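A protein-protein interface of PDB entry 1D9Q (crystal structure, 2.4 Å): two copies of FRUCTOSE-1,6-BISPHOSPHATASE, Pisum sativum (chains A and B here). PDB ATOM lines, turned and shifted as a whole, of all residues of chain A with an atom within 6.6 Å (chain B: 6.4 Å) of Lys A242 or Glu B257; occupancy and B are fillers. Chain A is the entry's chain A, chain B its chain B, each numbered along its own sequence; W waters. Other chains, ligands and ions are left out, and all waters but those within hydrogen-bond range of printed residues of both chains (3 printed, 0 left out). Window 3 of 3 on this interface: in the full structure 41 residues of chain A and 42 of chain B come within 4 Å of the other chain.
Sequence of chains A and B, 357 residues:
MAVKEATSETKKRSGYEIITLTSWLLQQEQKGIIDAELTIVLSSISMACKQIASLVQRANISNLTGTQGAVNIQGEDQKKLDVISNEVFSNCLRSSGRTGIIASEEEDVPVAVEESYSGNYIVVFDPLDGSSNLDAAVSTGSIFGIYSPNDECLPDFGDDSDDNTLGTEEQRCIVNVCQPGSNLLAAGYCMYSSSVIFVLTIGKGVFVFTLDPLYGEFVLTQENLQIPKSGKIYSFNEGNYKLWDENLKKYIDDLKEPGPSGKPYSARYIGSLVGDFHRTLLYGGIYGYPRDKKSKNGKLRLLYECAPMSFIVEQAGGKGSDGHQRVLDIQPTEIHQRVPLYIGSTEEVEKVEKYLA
Gly A239 touches Pro B264 (O to CG, 3.4 Å).
O of Tyr B265 touches CA of Gly A239, at 3.3 Å.
Asn A240 touches Pro B264.
Lys B256 touches Tyr A241 (CD to CB, 3.9 Å).
O of Lys B256 touches CB of Lys A242, 3.9 Å away.
The side-chain carboxylate (OE1) of Glu A238 is in salt-bridge range of the side-chain amino group (NZ) of Lys B256.
The side-chain amino group (NZ) of Lys A242 is in salt-bridge range of the side-chain carboxylate (OE2) of Glu B257 (2.9 Å).
N of Tyr B265 sits at hydrogen-bond distance from O of Leu B255, at 3.3 Å.
Water W2 lies within hydrogen-bond range of the side-chain amino group of Lys B256 (2.5 Å) and the side-chain carboxylate of Glu A238 (2.9 Å).
Water W3 lies within hydrogen-bond range of ND2 of Asn A240 (2.6 Å) and O of Tyr B265 (3.2 Å).
Water W1 lies within hydrogen-bond range of O of Gly A239, O of Lys B256, N of Lys A242 and N of Tyr A241.
Printed residues of chain A that touch a printed residue of chain B: Glu A238, Gly A239, Asn A240, Tyr A241 and Lys A242.
Hydrophobic or aromatic side chains of chain A within 4 Å of the printed part of chain B: Tyr A241.
Hydrophobic or aromatic side chains of chain B that line the printed part of chain A: Pro B264.
Along chain B the printed residues that touch a printed residue of chain A span positions 256 to 265.
Among the printed residues, 7 pairs touch across the chains.
Among the printed residues, Asp or Glu carboxylates within 4 Å of a Lys or Arg side-chain nitrogen of the other chain: Glu A238 with Lys B256 and Lys A242 with Glu B257.
Printed residues of chain B within 4 Å of Glu A238: Lys B256 (3.5 Å).
Of the printed residues of chain B, Gly A239 touches Pro B264 (3.4 Å) and Tyr B265 (3.3 Å).
Of the printed residues of chain B, Asn A240 touches Pro B264 (3.96 Å).
Of the printed residues of chain B, Tyr A241 touches Lys B256.
Lys A242 touches two residues of chain B.
Asp B253 touches none of the printed residues of chain A.
Glu B257 touches just one residue of chain A: Lys A242 (2.9 Å).
Pro B260 touches none of the printed residues of chain A.
Of the printed residues of chain A, Tyr B265 touches Gly A239 (3.3 Å).
The nearest residue of chain B that does not touch Lys A242 is Asp B253 (4.3 Å).
No position is printed for both chains.
Of the 7 pairs that touch across the chains among the printed residues, none has its exchanged pair printed and touching as well.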
ATOM      1  N   GLU A 238      34.034  27.629  -9.796  1.00  0.00           N
ATOM      2  CA  GLU A 238      32.589  27.507  -9.760  1.00  0.00           C
ATOM      3  C   GLU A 238      31.873  27.680 -11.067  1.00  0.00           C
ATOM      4  O   GLU A 238      30.654  27.550 -11.113  1.00  0.00           O
ATOM      5  CB  GLU A 238      31.980  28.420  -8.714  1.00  0.00           C
ATOM      6  CG  GLU A 238      32.063  27.846  -7.327  1.00  0.00           C
ATOM      7  CD  GLU A 238      31.072  28.479  -6.386  1.00  0.00           C
ATOM      8  OE1 GLU A 238      29.871  28.147  -6.481  1.00  0.00           O
ATOM      9  OE2 GLU A 238      31.494  29.296  -5.548  1.00  0.00           O
ATOM     10  N   GLY A 239      32.618  27.997 -12.119  1.00  0.00           N
ATOM     11  CA  GLY A 239      32.012  28.139 -13.429  1.00  0.00           C
ATOM     12  C   GLY A 239      31.511  26.781 -13.909  1.00  0.00           C
ATOM     13  O   GLY A 239      30.590  26.701 -14.708  1.00  0.00           O
ATOM     14  N   ASN A 240      32.121  25.710 -13.406  1.00  0.00           N
ATOM     15  CA  ASN A 240      31.750  24.342 -13.773  1.00  0.00           C
ATOM     16  C   ASN A 240      30.721  23.726 -12.831  1.00  0.00           C
ATOM     17  O   ASN A 240      30.522  22.519 -12.853  1.00  0.00           O
ATOM     18  CB  ASN A 240      32.976  23.431 -13.730  1.00  0.00           C
ATOM     19  CG  ASN A 240      33.996  23.764 -14.773  1.00  0.00           C
ATOM     20  OD1 ASN A 240      35.192  23.563 -14.561  1.00  0.00           O
ATOM     21  ND2 ASN A 240      33.537  24.256 -15.919  1.00  0.00           N
ATOM     22  N   TYR A 241      30.079  24.552 -12.015  1.00  0.00           N
ATOM     23  CA  TYR A 241      29.102  24.087 -11.036  1.00  0.00           C
ATOM     24  C   TYR A 241      28.056  23.096 -11.542  1.00  0.00           C
ATOM     25  O   TYR A 241      27.787  22.089 -10.890  1.00  0.00           O
ATOM     26  CB  TYR A 241      28.423  25.290 -10.382  1.00  0.00           C
ATOM     27  CG  TYR A 241      27.347  24.946  -9.369  1.00  0.00           C
ATOM     28  CD1 TYR A 241      27.686  24.606  -8.058  1.00  0.00           C
ATOM     29  CD2 TYR A 241      26.000  25.021  -9.721  1.00  0.00           C
ATOM     30  CE1 TYR A 241      26.698  24.356  -7.112  1.00  0.00           C
ATOM     31  CE2 TYR A 241      25.009  24.774  -8.783  1.00  0.00           C
ATOM     32  CZ  TYR A 241      25.356  24.442  -7.479  1.00  0.00           C
ATOM     33  OH  TYR A 241      24.368  24.200  -6.557  1.00  0.00           O
ATOM     34  N   LYS A 242      27.477  23.369 -12.704  1.00  0.00           N
ATOM     35  CA  LYS A 242      26.445  22.496 -13.260  1.00  0.00           C
ATOM     36  C   LYS A 242      26.959  21.221 -13.919  1.00  0.00           C
ATOM     37  O   LYS A 242      26.164  20.384 -14.350  1.00  0.00           O
ATOM     38  CB  LYS A 242      25.509  23.275 -14.187  1.00  0.00           C
ATOM     39  CG  LYS A 242      24.551  24.138 -13.370  1.00  0.00           C
ATOM     40  CD  LYS A 242      23.477  24.854 -14.181  1.00  0.00           C
ATOM     41  CE  LYS A 242      22.492  25.522 -13.201  1.00  0.00           C
ATOM     42  NZ  LYS A 242      21.462  26.379 -13.850  1.00  0.00           N
ATOM     43  N   LEU A 243      28.278  21.054 -13.941  1.00  0.00           N
ATOM     44  CA  LEU A 243      28.910  19.863 -14.500  1.00  0.00           C
ATOM     45  C   LEU A 243      29.342  18.914 -13.368  1.00  0.00           C
ATOM     46  O   LEU A 243      29.789  17.790 -13.619  1.00  0.00           O
ATOM     47  CB  LEU A 243      30.130  20.273 -15.328  1.00  0.00           C
ATOM     48  CG  LEU A 243      29.898  21.250 -16.480  1.00  0.00           C
ATOM     49  CD1 LEU A 243      31.229  21.589 -17.157  1.00  0.00           C
ATOM     50  CD2 LEU A 243      28.956  20.598 -17.482  1.00  0.00           C
ATOM     51  N   TRP A 244      29.201  19.379 -12.130  1.00  0.00           N
ATOM     52  CA  TRP A 244      29.570  18.603 -10.963  1.00  0.00           C
ATOM     53  C   TRP A 244      28.454  17.681 -10.510  1.00  0.00           C
ATOM     54  O   TRP A 244      27.300  17.864 -10.871  1.00  0.00           O
ATOM     55  CB  TRP A 244      29.962  19.535  -9.810  1.00  0.00           C
ATOM     56  CG  TRP A 244      31.250  20.291 -10.020  1.00  0.00           C
ATOM     57  CD1 TRP A 244      32.262  19.971 -10.878  1.00  0.00           C
ATOM     58  CD2 TRP A 244      31.648  21.501  -9.361  1.00  0.00           C
ATOM     59  NE1 TRP A 244      33.267  20.902 -10.792  1.00  0.00           N
ATOM     60  CE2 TRP A 244      32.920  21.849  -9.863  1.00  0.00           C
ATOM     61  CE3 TRP A 244      31.060  22.319  -8.382  1.00  0.00           C
ATOM     62  CZ2 TRP A 244      33.603  22.998  -9.443  1.00  0.00           C
ATOM     63  CZ3 TRP A 244      31.737  23.461  -7.963  1.00  0.00           C
ATOM     64  CH2 TRP A 244      32.997  23.783  -8.486  1.00  0.00           C
ATOM     65  N   ASP A 245      28.814  16.689  -9.707  1.00  0.00           N
ATOM     66  CA  ASP A 245      27.852  15.740  -9.169  1.00  0.00           C
ATOM     67  C   ASP A 245      27.027  16.425  -8.093  1.00  0.00           C
ATOM     68  O   ASP A 245      27.476  17.424  -7.506  1.00  0.00           O
ATOM     69  CB  ASP A 245      28.582  14.542  -8.558  1.00  0.00           C
ATOM     70  CG  ASP A 245      29.235  13.641  -9.610  1.00  0.00           C
ATOM     71  OD1 ASP A 245      29.022  13.836 -10.836  1.00  0.00           O
ATOM     72  OD2 ASP A 245      29.958  12.711  -9.190  1.00  0.00           O
ATOM     73  N   LYS A 249      27.856  19.602  -5.396  1.00  0.00           N
ATOM     74  CA  LYS A 249      27.045  20.814  -5.453  1.00  0.00           C
ATOM     75  C   LYS A 249      26.518  21.169  -4.072  1.00  0.00           C
ATOM     76  O   LYS A 249      26.494  22.329  -3.689  1.00  0.00           O
ATOM     77  CB  LYS A 249      25.867  20.632  -6.389  1.00  0.00           C
ATOM     78  CG  LYS A 249      26.210  20.521  -7.842  1.00  0.00           C
ATOM     79  CD  LYS A 249      24.923  20.611  -8.625  1.00  0.00           C
ATOM     80  CE  LYS A 249      25.088  20.369 -10.094  1.00  0.00           C
ATOM     81  NZ  LYS A 249      23.753  20.483 -10.765  1.00  0.00           N
ATOM     82  N   LYS A 293      31.217  15.660 -15.465  1.00  0.00           N
ATOM     83  CA  LYS A 293      30.601  14.841 -16.502  1.00  0.00           C
ATOM     84  C   LYS A 293      31.561  14.364 -17.600  1.00  0.00           C
ATOM     85  O   LYS A 293      31.677  13.162 -17.856  1.00  0.00           O
ATOM     86  CB  LYS A 293      29.438  15.616 -17.136  1.00  0.00           C
ATOM     87  CG  LYS A 293      28.071  15.367 -16.504  1.00  0.00           C
ATOM     88  CD  LYS A 293      27.694  13.882 -16.588  1.00  0.00           C
ATOM     89  CE  LYS A 293      26.186  13.655 -16.462  1.00  0.00           C
ATOM     90  NZ  LYS A 293      25.420  14.173 -17.647  1.00  0.00           N
ATOM     91  N   ILE B 252      24.293  35.505 -11.896  1.00  0.00           N
ATOM     92  CA  ILE B 252      25.355  34.561 -11.546  1.00  0.00           C
ATOM     93  C   ILE B 252      24.991  33.118 -11.925  1.00  0.00           C
ATOM     94  O   ILE B 252      25.819  32.387 -12.470  1.00  0.00           O
ATOM     95  CB  ILE B 252      25.723  34.671 -10.031  1.00  0.00           C
ATOM     96  CG1 ILE B 252      26.388  36.027  -9.737  1.00  0.00           C
ATOM     97  CG2 ILE B 252      26.649  33.546  -9.606  1.00  0.00           C
ATOM     98  CD1 ILE B 252      27.748  36.238 -10.396  1.00  0.00           C
ATOM     99  N   ASP B 253      23.737  32.738 -11.683  1.00  0.00           N
ATOM    100  CA  ASP B 253      23.241  31.394 -12.004  1.00  0.00           C
ATOM    101  C   ASP B 253      23.293  31.089 -13.488  1.00  0.00           C
ATOM    102  O   ASP B 253      23.711  30.002 -13.885  1.00  0.00           O
ATOM    103  CB  ASP B 253      21.800  31.223 -11.532  1.00  0.00           C
ATOM    104  CG  ASP B 253      21.672  31.182 -10.021  1.00  0.00           C
ATOM    105  OD1 ASP B 253      22.692  31.014  -9.306  1.00  0.00           O
ATOM    106  OD2 ASP B 253      20.527  31.318  -9.544  1.00  0.00           O
ATOM    107  N   ASP B 254      22.847  32.048 -14.296  1.00  0.00           N
ATOM    108  CA  ASP B 254      22.823  31.905 -15.746  1.00  0.00           C
ATOM    109  C   ASP B 254      24.193  31.802 -16.399  1.00  0.00           C
ATOM    110  O   ASP B 254      24.300  31.352 -17.538  1.00  0.00           O
ATOM    111  CB  ASP B 254      22.033  33.052 -16.391  1.00  0.00           C
ATOM    112  CG  ASP B 254      20.530  32.942 -16.160  1.00  0.00           C
ATOM    113  OD1 ASP B 254      20.075  31.938 -15.570  1.00  0.00           O
ATOM    114  OD2 ASP B 254      19.795  33.865 -16.569  1.00  0.00           O
ATOM    115  N   LEU B 255      25.234  32.258 -15.708  1.00  0.00           N
ATOM    116  CA  LEU B 255      26.585  32.188 -16.259  1.00  0.00           C
ATOM    117  C   LEU B 255      27.090  30.741 -16.222  1.00  0.00           C
ATOM    118  O   LEU B 255      27.977  30.362 -16.985  1.00  0.00           O
ATOM    119  CB  LEU B 255      27.538  33.099 -15.471  1.00  0.00           C
ATOM    120  CG  LEU B 255      27.258  34.598 -15.435  1.00  0.00           C
ATOM    121  CD1 LEU B 255      28.336  35.259 -14.635  1.00  0.00           C
ATOM    122  CD2 LEU B 255      27.199  35.187 -16.821  1.00  0.00           C
ATOM    123  N   LYS B 256      26.490  29.938 -15.347  1.00  0.00           N
ATOM    124  CA  LYS B 256      26.864  28.541 -15.174  1.00  0.00           C
ATOM    125  C   LYS B 256      26.209  27.607 -16.167  1.00  0.00           C
ATOM    126  O   LYS B 256      26.540  26.424 -16.226  1.00  0.00           O
ATOM    127  CB  LYS B 256      26.576  28.107 -13.746  1.00  0.00           C
ATOM    128  CG  LYS B 256      27.428  28.875 -12.774  1.00  0.00           C
ATOM    129  CD  LYS B 256      26.969  28.729 -11.367  1.00  0.00           C
ATOM    130  CE  LYS B 256      27.866  29.544 -10.475  1.00  0.00           C
ATOM    131  NZ  LYS B 256      27.442  29.423  -9.063  1.00  0.00           N
ATOM    132  N   GLU B 257      25.286  28.158 -16.953  1.00  0.00           N
ATOM    133  CA  GLU B 257      24.571  27.420 -17.995  1.00  0.00           C
ATOM    134  C   GLU B 257      25.445  27.213 -19.224  1.00  0.00           C
ATOM    135  O   GLU B 257      25.845  28.177 -19.882  1.00  0.00           O
ATOM    136  CB  GLU B 257      23.310  28.183 -18.409  1.00  0.00           C
ATOM    137  CG  GLU B 257      22.103  27.912 -17.536  1.00  0.00           C
ATOM    138  CD  GLU B 257      21.585  26.488 -17.687  1.00  0.00           C
ATOM    139  OE1 GLU B 257      21.643  25.929 -18.816  1.00  0.00           O
ATOM    140  OE2 GLU B 257      21.118  25.933 -16.666  1.00  0.00           O
ATOM    141  N   PRO B 258      25.790  25.953 -19.533  1.00  0.00           N
ATOM    142  CA  PRO B 258      26.619  25.724 -20.706  1.00  0.00           C
ATOM    143  C   PRO B 258      25.835  26.126 -21.947  1.00  0.00           C
ATOM    144  O   PRO B 258      24.826  25.524 -22.316  1.00  0.00           O
ATOM    145  CB  PRO B 258      26.975  24.236 -20.584  1.00  0.00           C
ATOM    146  CG  PRO B 258      25.826  23.671 -19.826  1.00  0.00           C
ATOM    147  CD  PRO B 258      25.653  24.718 -18.747  1.00  0.00           C
ATOM    148  N   GLY B 259      26.253  27.240 -22.517  1.00  0.00           N
ATOM    149  CA  GLY B 259      25.564  27.744 -23.680  1.00  0.00           C
ATOM    150  C   GLY B 259      25.739  26.919 -24.916  1.00  0.00           C
ATOM    151  O   GLY B 259      25.185  25.811 -25.021  1.00  0.00           O
ATOM    152  N   PRO B 260      26.607  27.412 -25.822  1.00  0.00           N
ATOM    153  CA  PRO B 260      27.027  26.945 -27.122  1.00  0.00           C
ATOM    154  C   PRO B 260      27.686  25.606 -27.189  1.00  0.00           C
ATOM    155  O   PRO B 260      27.008  24.559 -27.138  1.00  0.00           O
ATOM    156  CB  PRO B 260      28.000  28.039 -27.553  1.00  0.00           C
ATOM    157  CG  PRO B 260      28.708  28.402 -26.316  1.00  0.00           C
ATOM    158  CD  PRO B 260      27.493  28.505 -25.365  1.00  0.00           C
ATOM    159  N   LYS B 263      30.007  24.848 -23.218  1.00  0.00           N
ATOM    160  CA  LYS B 263      31.055  25.390 -22.358  1.00  0.00           C
ATOM    161  C   LYS B 263      30.549  26.609 -21.579  1.00  0.00           C
ATOM    162  O   LYS B 263      30.187  27.635 -22.169  1.00  0.00           O
ATOM    163  CB  LYS B 263      32.273  25.772 -23.190  1.00  0.00           C
ATOM    164  N   PRO B 264      30.450  26.490 -20.246  1.00  0.00           N
ATOM    165  CA  PRO B 264      29.979  27.611 -19.428  1.00  0.00           C
ATOM    166  C   PRO B 264      31.102  28.630 -19.202  1.00  0.00           C
ATOM    167  O   PRO B 264      32.215  28.470 -19.714  1.00  0.00           O
ATOM    168  CB  PRO B 264      29.567  26.919 -18.126  1.00  0.00           C
ATOM    169  CG  PRO B 264      30.555  25.803 -18.022  1.00  0.00           C
ATOM    170  CD  PRO B 264      30.621  25.275 -19.431  1.00  0.00           C
ATOM    171  N   TYR B 265      30.801  29.683 -18.448  1.00  0.00           N
ATOM    172  CA  TYR B 265      31.799  30.706 -18.140  1.00  0.00           C
ATOM    173  C   TYR B 265      32.871  30.152 -17.214  1.00  0.00           C
ATOM    174  O   TYR B 265      32.606  29.239 -16.432  1.00  0.00           O
ATOM    175  CB  TYR B 265      31.145  31.888 -17.426  1.00  0.00           C
ATOM    176  CG  TYR B 265      30.568  32.948 -18.319  1.00  0.00           C
ATOM    177  CD1 TYR B 265      29.575  32.650 -19.237  1.00  0.00           C
ATOM    178  CD2 TYR B 265      30.996  34.262 -18.217  1.00  0.00           C
ATOM    179  CE1 TYR B 265      29.017  33.637 -20.031  1.00  0.00           C
ATOM    180  CE2 TYR B 265      30.450  35.260 -19.000  1.00  0.00           C
ATOM    181  CZ  TYR B 265      29.456  34.945 -19.906  1.00  0.00           C
ATOM    182  OH  TYR B 265      28.886  35.943 -20.668  1.00  0.00           O
HETATM  183  O   HOH W   1      28.430  25.120 -14.711  1.00  0.00           O
HETATM  184  O   HOH W   2      27.090  27.852  -7.119  1.00  0.00           O
HETATM  185  O   HOH W   3      34.399  26.640 -16.554  1.00  0.00           O
